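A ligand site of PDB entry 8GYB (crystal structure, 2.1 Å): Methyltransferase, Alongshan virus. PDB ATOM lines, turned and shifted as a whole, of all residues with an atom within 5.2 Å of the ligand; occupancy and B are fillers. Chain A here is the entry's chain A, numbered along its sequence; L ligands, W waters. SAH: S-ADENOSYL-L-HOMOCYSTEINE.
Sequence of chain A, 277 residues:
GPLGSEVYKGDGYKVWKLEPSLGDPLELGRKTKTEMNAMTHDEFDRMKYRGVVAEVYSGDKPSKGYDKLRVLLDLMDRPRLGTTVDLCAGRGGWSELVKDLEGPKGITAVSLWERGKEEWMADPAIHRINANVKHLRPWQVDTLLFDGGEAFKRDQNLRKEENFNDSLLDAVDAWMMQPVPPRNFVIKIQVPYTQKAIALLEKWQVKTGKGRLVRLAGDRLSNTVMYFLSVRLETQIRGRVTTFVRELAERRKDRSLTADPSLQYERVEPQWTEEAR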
ATOM      1  N   SER A  63       7.600 -15.123 -27.620  1.00  0.00           N
ATOM      2  CA  SER A  63       6.998 -14.761 -26.351  1.00  0.00           C
ATOM      3  C   SER A  63       5.574 -15.300 -26.317  1.00  0.00           C
ATOM      4  O   SER A  63       5.003 -15.659 -27.362  1.00  0.00           O
ATOM      5  CB  SER A  63       6.996 -13.232 -26.144  1.00  0.00           C
ATOM      6  OG  SER A  63       5.736 -12.763 -25.686  1.00  0.00           O
ATOM      7  N   LYS A  64       4.987 -15.350 -25.120  1.00  0.00           N
ATOM      8  CA  LYS A  64       3.618 -15.837 -24.992  1.00  0.00           C
ATOM      9  C   LYS A  64       2.606 -14.799 -25.465  1.00  0.00           C
ATOM     10  O   LYS A  64       1.492 -15.172 -25.888  1.00  0.00           O
ATOM     11  CB  LYS A  64       3.335 -16.246 -23.550  1.00  0.00           C
ATOM     12  CG  LYS A  64       2.014 -16.992 -23.374  1.00  0.00           C
ATOM     13  CD  LYS A  64       0.902 -16.067 -22.921  1.00  0.00           C
ATOM     14  CE  LYS A  64      -0.435 -16.791 -22.757  1.00  0.00           C
ATOM     15  NZ  LYS A  64      -1.118 -17.029 -24.055  1.00  0.00           N
ATOM     16  N   GLY A  65       2.964 -13.515 -25.418  1.00  0.00           N
ATOM     17  CA  GLY A  65       2.047 -12.485 -25.870  1.00  0.00           C
ATOM     18  C   GLY A  65       1.483 -12.732 -27.258  1.00  0.00           C
ATOM     19  O   GLY A  65       0.337 -12.361 -27.534  1.00  0.00           O
ATOM     20  N   TYR A  66       2.269 -13.369 -28.134  1.00  0.00           N
ATOM     21  CA  TYR A  66       1.805 -13.756 -29.458  1.00  0.00           C
ATOM     22  C   TYR A  66       0.402 -14.357 -29.369  1.00  0.00           C
ATOM     23  O   TYR A  66      -0.574 -13.789 -29.899  1.00  0.00           O
ATOM     24  CB  TYR A  66       2.798 -14.750 -30.068  1.00  0.00           C
ATOM     25  CG  TYR A  66       2.583 -15.084 -31.537  1.00  0.00           C
ATOM     26  CD1 TYR A  66       1.645 -16.033 -31.923  1.00  0.00           C
ATOM     27  CD2 TYR A  66       3.345 -14.488 -32.537  1.00  0.00           C
ATOM     28  CE1 TYR A  66       1.450 -16.348 -33.246  1.00  0.00           C
ATOM     29  CE2 TYR A  66       3.152 -14.814 -33.873  1.00  0.00           C
ATOM     30  CZ  TYR A  66       2.204 -15.739 -34.221  1.00  0.00           C
ATOM     31  OH  TYR A  66       1.989 -16.078 -35.534  1.00  0.00           O
ATOM     32  N   ASP A  86       3.401  -0.657 -32.005  1.00  0.00           N
ATOM     33  CA  ASP A  86       3.317  -1.585 -30.873  1.00  0.00           C
ATOM     34  C   ASP A  86       4.140  -0.960 -29.749  1.00  0.00           C
ATOM     35  O   ASP A  86       5.364  -1.038 -29.729  1.00  0.00           O
ATOM     36  CB  ASP A  86       3.809  -2.980 -31.288  1.00  0.00           C
ATOM     37  CG  ASP A  86       3.837  -3.993 -30.145  1.00  0.00           C
ATOM     38  OD1 ASP A  86       3.164  -3.831 -29.114  1.00  0.00           O
ATOM     39  OD2 ASP A  86       4.541  -5.011 -30.346  1.00  0.00           O
ATOM     40  N   CYS A  88       5.595  -0.391 -25.993  1.00  0.00           N
ATOM     41  CA  CYS A  88       6.124  -1.316 -24.988  1.00  0.00           C
ATOM     42  C   CYS A  88       6.200  -2.731 -25.582  1.00  0.00           C
ATOM     43  O   CYS A  88       5.612  -3.689 -25.072  1.00  0.00           O
ATOM     44  CB  CYS A  88       5.285  -1.275 -23.697  1.00  0.00           C
ATOM     45  SG  CYS A  88       5.268   0.360 -22.900  1.00  0.00           S
ATOM     46  N   ALA A  89       6.906  -2.821 -26.699  1.00  0.00           N
ATOM     47  CA  ALA A  89       6.911  -4.040 -27.497  1.00  0.00           C
ATOM     48  C   ALA A  89       7.634  -5.183 -26.819  1.00  0.00           C
ATOM     49  O   ALA A  89       7.363  -6.349 -27.141  1.00  0.00           O
ATOM     50  CB  ALA A  89       7.536  -3.765 -28.862  1.00  0.00           C
ATOM     51  N   GLY A  90       8.541  -4.890 -25.890  1.00  0.00           N
ATOM     52  CA  GLY A  90       9.177  -5.938 -25.122  1.00  0.00           C
ATOM     53  C   GLY A  90       9.932  -6.899 -26.020  1.00  0.00           C
ATOM     54  O   GLY A  90      10.725  -6.494 -26.880  1.00  0.00           O
ATOM     55  N   ARG A  91       9.682  -8.187 -25.830  1.00  0.00           N
ATOM     56  CA  ARG A  91      10.384  -9.202 -26.592  1.00  0.00           C
ATOM     57  C   ARG A  91       9.835  -9.387 -27.991  1.00  0.00           C
ATOM     58  O   ARG A  91      10.507 -10.003 -28.818  1.00  0.00           O
ATOM     59  CB  ARG A  91      10.330 -10.506 -25.830  1.00  0.00           C
ATOM     60  CG  ARG A  91      10.698 -10.285 -24.397  1.00  0.00           C
ATOM     61  CD  ARG A  91      11.662 -11.349 -23.962  1.00  0.00           C
ATOM     62  NE  ARG A  91      11.073 -12.687 -23.952  1.00  0.00           N
ATOM     63  CZ  ARG A  91      10.581 -13.267 -22.858  1.00  0.00           C
ATOM     64  NH1 ARG A  91      10.596 -12.634 -21.690  1.00  0.00           N
ATOM     65  NH2 ARG A  91      10.092 -14.490 -22.937  1.00  0.00           N
ATOM     66  N   GLY A  92       8.638  -8.864 -28.265  1.00  0.00           N
ATOM     67  CA  GLY A  92       8.142  -8.741 -29.618  1.00  0.00           C
ATOM     68  C   GLY A  92       7.066  -9.724 -30.056  1.00  0.00           C
ATOM     69  O   GLY A  92       6.821  -9.843 -31.263  1.00  0.00           O
ATOM     70  N   GLY A  93       6.429 -10.427 -29.115  1.00  0.00           N
ATOM     71  CA  GLY A  93       5.401 -11.384 -29.515  1.00  0.00           C
ATOM     72  C   GLY A  93       4.281 -10.743 -30.323  1.00  0.00           C
ATOM     73  O   GLY A  93       3.833 -11.297 -31.331  1.00  0.00           O
ATOM     74  N   TRP A  94       3.825  -9.564 -29.889  1.00  0.00           N
ATOM     75  CA  TRP A  94       2.747  -8.876 -30.601  1.00  0.00           C
ATOM     76  C   TRP A  94       3.199  -8.428 -31.976  1.00  0.00           C
ATOM     77  O   TRP A  94       2.503  -8.643 -32.985  1.00  0.00           O
ATOM     78  CB  TRP A  94       2.245  -7.691 -29.770  1.00  0.00           C
ATOM     79  CG  TRP A  94       1.389  -8.095 -28.603  1.00  0.00           C
ATOM     80  CD1 TRP A  94       1.326  -9.331 -28.013  1.00  0.00           C
ATOM     81  CD2 TRP A  94       0.451  -7.268 -27.884  1.00  0.00           C
ATOM     82  NE1 TRP A  94       0.415  -9.315 -26.984  1.00  0.00           N
ATOM     83  CE2 TRP A  94      -0.132  -8.064 -26.881  1.00  0.00           C
ATOM     84  CE3 TRP A  94       0.054  -5.925 -28.001  1.00  0.00           C
ATOM     85  CZ2 TRP A  94      -1.087  -7.565 -25.989  1.00  0.00           C
ATOM     86  CZ3 TRP A  94      -0.895  -5.429 -27.121  1.00  0.00           C
ATOM     87  CH2 TRP A  94      -1.456  -6.246 -26.127  1.00  0.00           C
ATOM     88  N   VAL A 110       8.104  -0.207 -30.370  1.00  0.00           N
ATOM     89  CA  VAL A 110       8.708   0.790 -29.497  1.00  0.00           C
ATOM     90  C   VAL A 110       8.877   0.200 -28.104  1.00  0.00           C
ATOM     91  O   VAL A 110       7.902  -0.262 -27.510  1.00  0.00           O
ATOM     92  CB  VAL A 110       7.859   2.081 -29.416  1.00  0.00           C
ATOM     93  CG1 VAL A 110       8.608   3.148 -28.641  1.00  0.00           C
ATOM     94  CG2 VAL A 110       7.484   2.576 -30.797  1.00  0.00           C
ATOM     95  N   SER A 111      10.098   0.243 -27.587  1.00  0.00           N
ATOM     96  CA  SER A 111      10.368  -0.271 -26.251  1.00  0.00           C
ATOM     97  C   SER A 111      11.721   0.255 -25.792  1.00  0.00           C
ATOM     98  O   SER A 111      12.500   0.775 -26.583  1.00  0.00           O
ATOM     99  CB  SER A 111      10.327  -1.800 -26.229  1.00  0.00           C
ATOM    100  OG  SER A 111       9.959  -2.273 -24.950  1.00  0.00           O
ATOM    101  N   LEU A 112      11.983   0.114 -24.488  1.00  0.00           N
ATOM    102  CA  LEU A 112      13.300   0.394 -23.898  1.00  0.00           C
ATOM    103  C   LEU A 112      14.047  -0.924 -23.744  1.00  0.00           C
ATOM    104  O   LEU A 112      13.668  -1.774 -22.931  1.00  0.00           O
ATOM    105  CB  LEU A 112      13.166   1.076 -22.542  1.00  0.00           C
ATOM    106  CG  LEU A 112      12.800   2.549 -22.439  1.00  0.00           C
ATOM    107  CD1 LEU A 112      12.670   2.931 -20.961  1.00  0.00           C
ATOM    108  CD2 LEU A 112      13.857   3.386 -23.115  1.00  0.00           C
ATOM    109  N   GLU A 118      12.607  -6.666 -22.914  1.00  0.00           N
ATOM    110  CA  GLU A 118      13.995  -7.014 -22.683  1.00  0.00           C
ATOM    111  C   GLU A 118      14.075  -8.525 -22.819  1.00  0.00           C
ATOM    112  O   GLU A 118      13.669  -9.266 -21.934  1.00  0.00           O
ATOM    113  CB  GLU A 118      14.465  -6.556 -21.304  1.00  0.00           C
ATOM    114  CG  GLU A 118      13.565  -5.542 -20.614  1.00  0.00           C
ATOM    115  CD  GLU A 118      12.180  -6.075 -20.285  1.00  0.00           C
ATOM    116  OE1 GLU A 118      11.668  -5.789 -19.197  1.00  0.00           O
ATOM    117  OE2 GLU A 118      11.595  -6.779 -21.119  1.00  0.00           O
ATOM    118  N   ALA A 131      12.970   3.714 -27.454  1.00  0.00           N
ATOM    119  CA  ALA A 131      12.574   4.967 -26.838  1.00  0.00           C
ATOM    120  C   ALA A 131      11.584   4.698 -25.719  1.00  0.00           C
ATOM    121  O   ALA A 131      10.921   3.659 -25.681  1.00  0.00           O
ATOM    122  CB  ALA A 131      11.949   5.924 -27.869  1.00  0.00           C
ATOM    123  N   ASN A 132      11.512   5.666 -24.805  1.00  0.00           N
ATOM    124  CA  ASN A 132      10.517   5.656 -23.744  1.00  0.00           C
ATOM    125  C   ASN A 132       9.188   6.133 -24.324  1.00  0.00           C
ATOM    126  O   ASN A 132       9.114   7.243 -24.851  1.00  0.00           O
ATOM    127  CB  ASN A 132      10.977   6.565 -22.599  1.00  0.00           C
ATOM    128  CG  ASN A 132      10.142   6.402 -21.343  1.00  0.00           C
ATOM    129  OD1 ASN A 132       8.978   5.996 -21.397  1.00  0.00           O
ATOM    130  ND2 ASN A 132      10.739   6.725 -20.196  1.00  0.00           N
ATOM    131  N   VAL A 133       8.149   5.301 -24.226  1.00  0.00           N
ATOM    132  CA  VAL A 133       6.850   5.648 -24.799  1.00  0.00           C
ATOM    133  C   VAL A 133       6.290   6.935 -24.205  1.00  0.00           C
ATOM    134  O   VAL A 133       5.397   7.545 -24.795  1.00  0.00           O
ATOM    135  CB  VAL A 133       5.849   4.481 -24.634  1.00  0.00           C
ATOM    136  CG1 VAL A 133       6.326   3.245 -25.388  1.00  0.00           C
ATOM    137  CG2 VAL A 133       5.620   4.166 -23.172  1.00  0.00           C
ATOM    138  N   LYS A 134       6.793   7.365 -23.047  1.00  0.00           N
ATOM    139  CA  LYS A 134       6.343   8.628 -22.470  1.00  0.00           C
ATOM    140  C   LYS A 134       6.941   9.831 -23.190  1.00  0.00           C
ATOM    141  O   LYS A 134       6.324  10.904 -23.205  1.00  0.00           O
ATOM    142  CB  LYS A 134       6.685   8.687 -20.973  1.00  0.00           C
ATOM    143  CG  LYS A 134       6.062   7.588 -20.131  1.00  0.00           C
ATOM    144  CD  LYS A 134       6.477   7.725 -18.674  1.00  0.00           C
ATOM    145  CE  LYS A 134       6.042   6.527 -17.851  1.00  0.00           C
ATOM    146  NZ  LYS A 134       6.552   6.607 -16.446  1.00  0.00           N
ATOM    147  N   ASP A 147       1.071  -2.944 -24.685  1.00  0.00           N
ATOM    148  CA  ASP A 147       1.127  -4.063 -23.759  1.00  0.00           C
ATOM    149  C   ASP A 147       2.027  -3.735 -22.581  1.00  0.00           C
ATOM    150  O   ASP A 147       2.696  -4.609 -22.022  1.00  0.00           O
ATOM    151  CB  ASP A 147       1.602  -5.339 -24.458  1.00  0.00           C
ATOM    152  CG  ASP A 147       1.356  -6.605 -23.627  1.00  0.00           C
ATOM    153  OD1 ASP A 147       0.346  -6.662 -22.907  1.00  0.00           O
ATOM    154  OD2 ASP A 147       2.191  -7.536 -23.700  1.00  0.00           O
ATOM    155  N   GLY A 148       2.067  -2.464 -22.198  1.00  0.00           N
ATOM    156  CA  GLY A 148       2.834  -2.085 -21.044  1.00  0.00           C
ATOM    157  C   GLY A 148       2.051  -2.255 -19.759  1.00  0.00           C
ATOM    158  O   GLY A 148       0.819  -2.369 -19.756  1.00  0.00           O
ATOM    159  N   GLU A 150       2.939  -3.329 -15.258  1.00  0.00           N
ATOM    160  CA  GLU A 150       3.634  -4.272 -14.396  1.00  0.00           C
ATOM    161  C   GLU A 150       2.842  -4.438 -13.108  1.00  0.00           C
ATOM    162  O   GLU A 150       2.386  -3.445 -12.526  1.00  0.00           O
ATOM    163  CB  GLU A 150       5.062  -3.806 -14.081  1.00  0.00           C
ATOM    164  CG  GLU A 150       5.931  -3.451 -15.281  1.00  0.00           C
ATOM    165  CD  GLU A 150       6.260  -4.640 -16.171  1.00  0.00           C
ATOM    166  OE1 GLU A 150       6.002  -5.797 -15.773  1.00  0.00           O
ATOM    167  OE2 GLU A 150       6.786  -4.417 -17.287  1.00  0.00           O
ATOM    168  N   PHE A 164       2.346   4.109 -10.995  1.00  0.00           N
ATOM    169  CA  PHE A 164       3.202   3.628 -12.082  1.00  0.00           C
ATOM    170  C   PHE A 164       2.363   3.295 -13.316  1.00  0.00           C
ATOM    171  O   PHE A 164       2.646   3.773 -14.430  1.00  0.00           O
ATOM    172  CB  PHE A 164       3.997   2.409 -11.603  1.00  0.00           C
ATOM    173  CG  PHE A 164       4.891   1.802 -12.663  1.00  0.00           C
ATOM    174  CD1 PHE A 164       4.393   0.849 -13.528  1.00  0.00           C
ATOM    175  CD2 PHE A 164       6.224   2.158 -12.769  1.00  0.00           C
ATOM    176  CE1 PHE A 164       5.194   0.283 -14.506  1.00  0.00           C
ATOM    177  CE2 PHE A 164       7.037   1.583 -13.731  1.00  0.00           C
ATOM    178  CZ  PHE A 164       6.517   0.643 -14.610  1.00  0.00           C
ATOM    179  N   LEU A 168       1.984   5.144 -17.149  1.00  0.00           N
ATOM    180  CA  LEU A 168       2.131   4.434 -18.419  1.00  0.00           C
ATOM    181  C   LEU A 168       0.930   4.663 -19.341  1.00  0.00           C
ATOM    182  O   LEU A 168       1.097   4.961 -20.533  1.00  0.00           O
ATOM    183  CB  LEU A 168       2.340   2.941 -18.181  1.00  0.00           C
ATOM    184  CG  LEU A 168       3.782   2.479 -18.111  1.00  0.00           C
ATOM    185  CD1 LEU A 168       3.814   0.968 -18.216  1.00  0.00           C
ATOM    186  CD2 LEU A 168       4.619   3.125 -19.211  1.00  0.00           C
HETATM  187  N   SAH L   1       3.808  -7.584 -25.749  1.00  0.00           N
HETATM  188  CA  SAH L   1       5.162  -8.092 -25.556  1.00  0.00           C
HETATM  189  CB  SAH L   1       5.587  -7.983 -24.097  1.00  0.00           C
HETATM  190  CG  SAH L   1       5.333  -6.626 -23.457  1.00  0.00           C
HETATM  191  SD  SAH L   1       6.166  -6.580 -21.856  1.00  0.00           S
HETATM  192  C   SAH L   1       5.342  -9.514 -26.069  1.00  0.00           C
HETATM  193  O   SAH L   1       6.446 -10.045 -26.112  1.00  0.00           O
HETATM  194  OXT SAH L   1       4.386 -10.167 -26.471  1.00  0.00           O
HETATM  195  C5' SAH L   1       6.188  -4.766 -21.770  1.00  0.00           C
HETATM  196  C4' SAH L   1       7.535  -4.161 -22.150  1.00  0.00           C
HETATM  197  O4' SAH L   1       7.455  -2.751 -22.036  1.00  0.00           O
HETATM  198  C3' SAH L   1       8.676  -4.596 -21.239  1.00  0.00           C
HETATM  199  O3' SAH L   1       9.612  -5.338 -21.991  1.00  0.00           O
HETATM  200  C2' SAH L   1       9.345  -3.318 -20.757  1.00  0.00           C
HETATM  201  O2' SAH L   1      10.727  -3.395 -21.009  1.00  0.00           O
HETATM  202  C1' SAH L   1       8.711  -2.249 -21.625  1.00  0.00           C
HETATM  203  N9  SAH L   1       8.523  -0.941 -20.958  1.00  0.00           N
HETATM  204  C8  SAH L   1       8.145  -0.681 -19.663  1.00  0.00           C
HETATM  205  N7  SAH L   1       8.103   0.658 -19.500  1.00  0.00           N
HETATM  206  C5  SAH L   1       8.439   1.250 -20.664  1.00  0.00           C
HETATM  207  C6  SAH L   1       8.556   2.585 -21.056  1.00  0.00           C
HETATM  208  N6  SAH L   1       8.311   3.573 -20.206  1.00  0.00           N
HETATM  209  N1  SAH L   1       8.929   2.874 -22.356  1.00  0.00           N
HETATM  210  C2  SAH L   1       9.191   1.859 -23.257  1.00  0.00           C
HETATM  211  N3  SAH L   1       9.075   0.546 -22.860  1.00  0.00           N
HETATM  212  C4  SAH L   1       8.700   0.250 -21.593  1.00  0.00           C
HETATM  213  O   HOH W   1      11.716  -3.767 -23.280  1.00  0.00           O
HETATM  214  O   HOH W   2       7.485   3.371 -17.207  1.00  0.00           O
HETATM  215  O   HOH W   3       5.380  -7.212 -28.867  1.00  0.00           O
HETATM  216  O   HOH W   4       5.829  -2.591 -18.614  1.00  0.00           O
HETATM  217  O   HOH W   5       3.612  -4.911 -26.977  1.00  0.00           O
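The backbone NH of Lys 134 sits close to the side-chain amide oxygen of Asn 132, 3.1 Å away. The side-chain hydroxyl (OG) of Ser 63 is in hydrogen-bond range of the backbone NH (N) of Gly 65 (2.9 Å). The backbone NH (N) of Cys 88 is in hydrogen-bond range of the backbone carbonyl oxygen (O) of Val 110 (2.8 Å). OG of Ser 111 is in hydrogen-bond range of N of Gly 90, 3.1 Å away. The backbone carbonyl oxygen (O) of Val 110 is in hydrogen-bond range of the backbone NH (N) of Ala 89. O of Gly 65 lies within hydrogen-bond range of NE1 of Trp 94, at 3.1 Å. The backbone NH (N) of Ala 131 is in hydrogen-bond range of the backbone carbonyl oxygen (O) of Ser 111.
Water W1 lies within hydrogen-bond range of O2' of the ligand (2.5 Å), O of Leu 112 (2.8 Å), OG of Ser 111 (2.8 Å) and N of Glu 118 (3.1 Å). Water W5 lies within hydrogen-bond range of the side-chain carboxylate of Asp 86 (2.4 Å), a nitrogen (N) of the ligand (2.9 Å) and the backbone carbonyl oxygen of Cys 88 (3.0 Å). Water W2 bridges a nitrogen (N6) of the ligand (3.1 Å) and the side-chain amino group (NZ) of Lys 134 (3.5 Å). Water W3 lies within hydrogen-bond range of the backbone carbonyl oxygen (O) of Ala 89, the side-chain carboxylate (OD2) of Asp 86, the backbone NH (N) of Trp 94 and the backbone NH (N) of Gly 93.
N of Glu 118 sits close to O3' of the ligand (3.4 Å). The side-chain carboxylate (OE2) of Glu 118 is in hydrogen-bond range of an oxygen (O3') of the ligand, at 2.6 Å. A nitrogen (N) of the ligand is in salt-bridge range of the side-chain carboxylate of Asp 147, 2.6 Å away. OD1 of Asn 132 is in hydrogen-bond range of N6 of the ligand, 2.8 Å away. O of the ligand sits at hydrogen-bond distance from OG of Ser 63 (2.8 Å). The backbone NH of Gly 93 lies within hydrogen-bond range of an oxygen (O) of the ligand (3.0 Å). The backbone NH (N) of Val 133 sits at hydrogen-bond distance from a nitrogen (N1) of the ligand, 3.2 Å away. The backbone NH (N) of Gly 92 is in hydrogen-bond range of an oxygen (O) of the ligand. A nitrogen (N3) of the ligand lies within hydrogen-bond range of the backbone NH (N) of Leu 112 (3.4 Å).
Residues that only touch the ligand: Cys 88, Gly 90, Ala 89, Gly 65, Ala 131, Trp 94, Ser 111, Arg 91 and Leu 168. 17 residues have an atom within 4 Å of the ligand: Ser 63, Gly 65, Cys 88, Ala 89, Gly 90, Arg 91, Gly 92, Gly 93, Trp 94, Ser 111, Leu 112, Glu 118, Ala 131, Asn 132, Val 133, Asp 147 and Leu 168.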
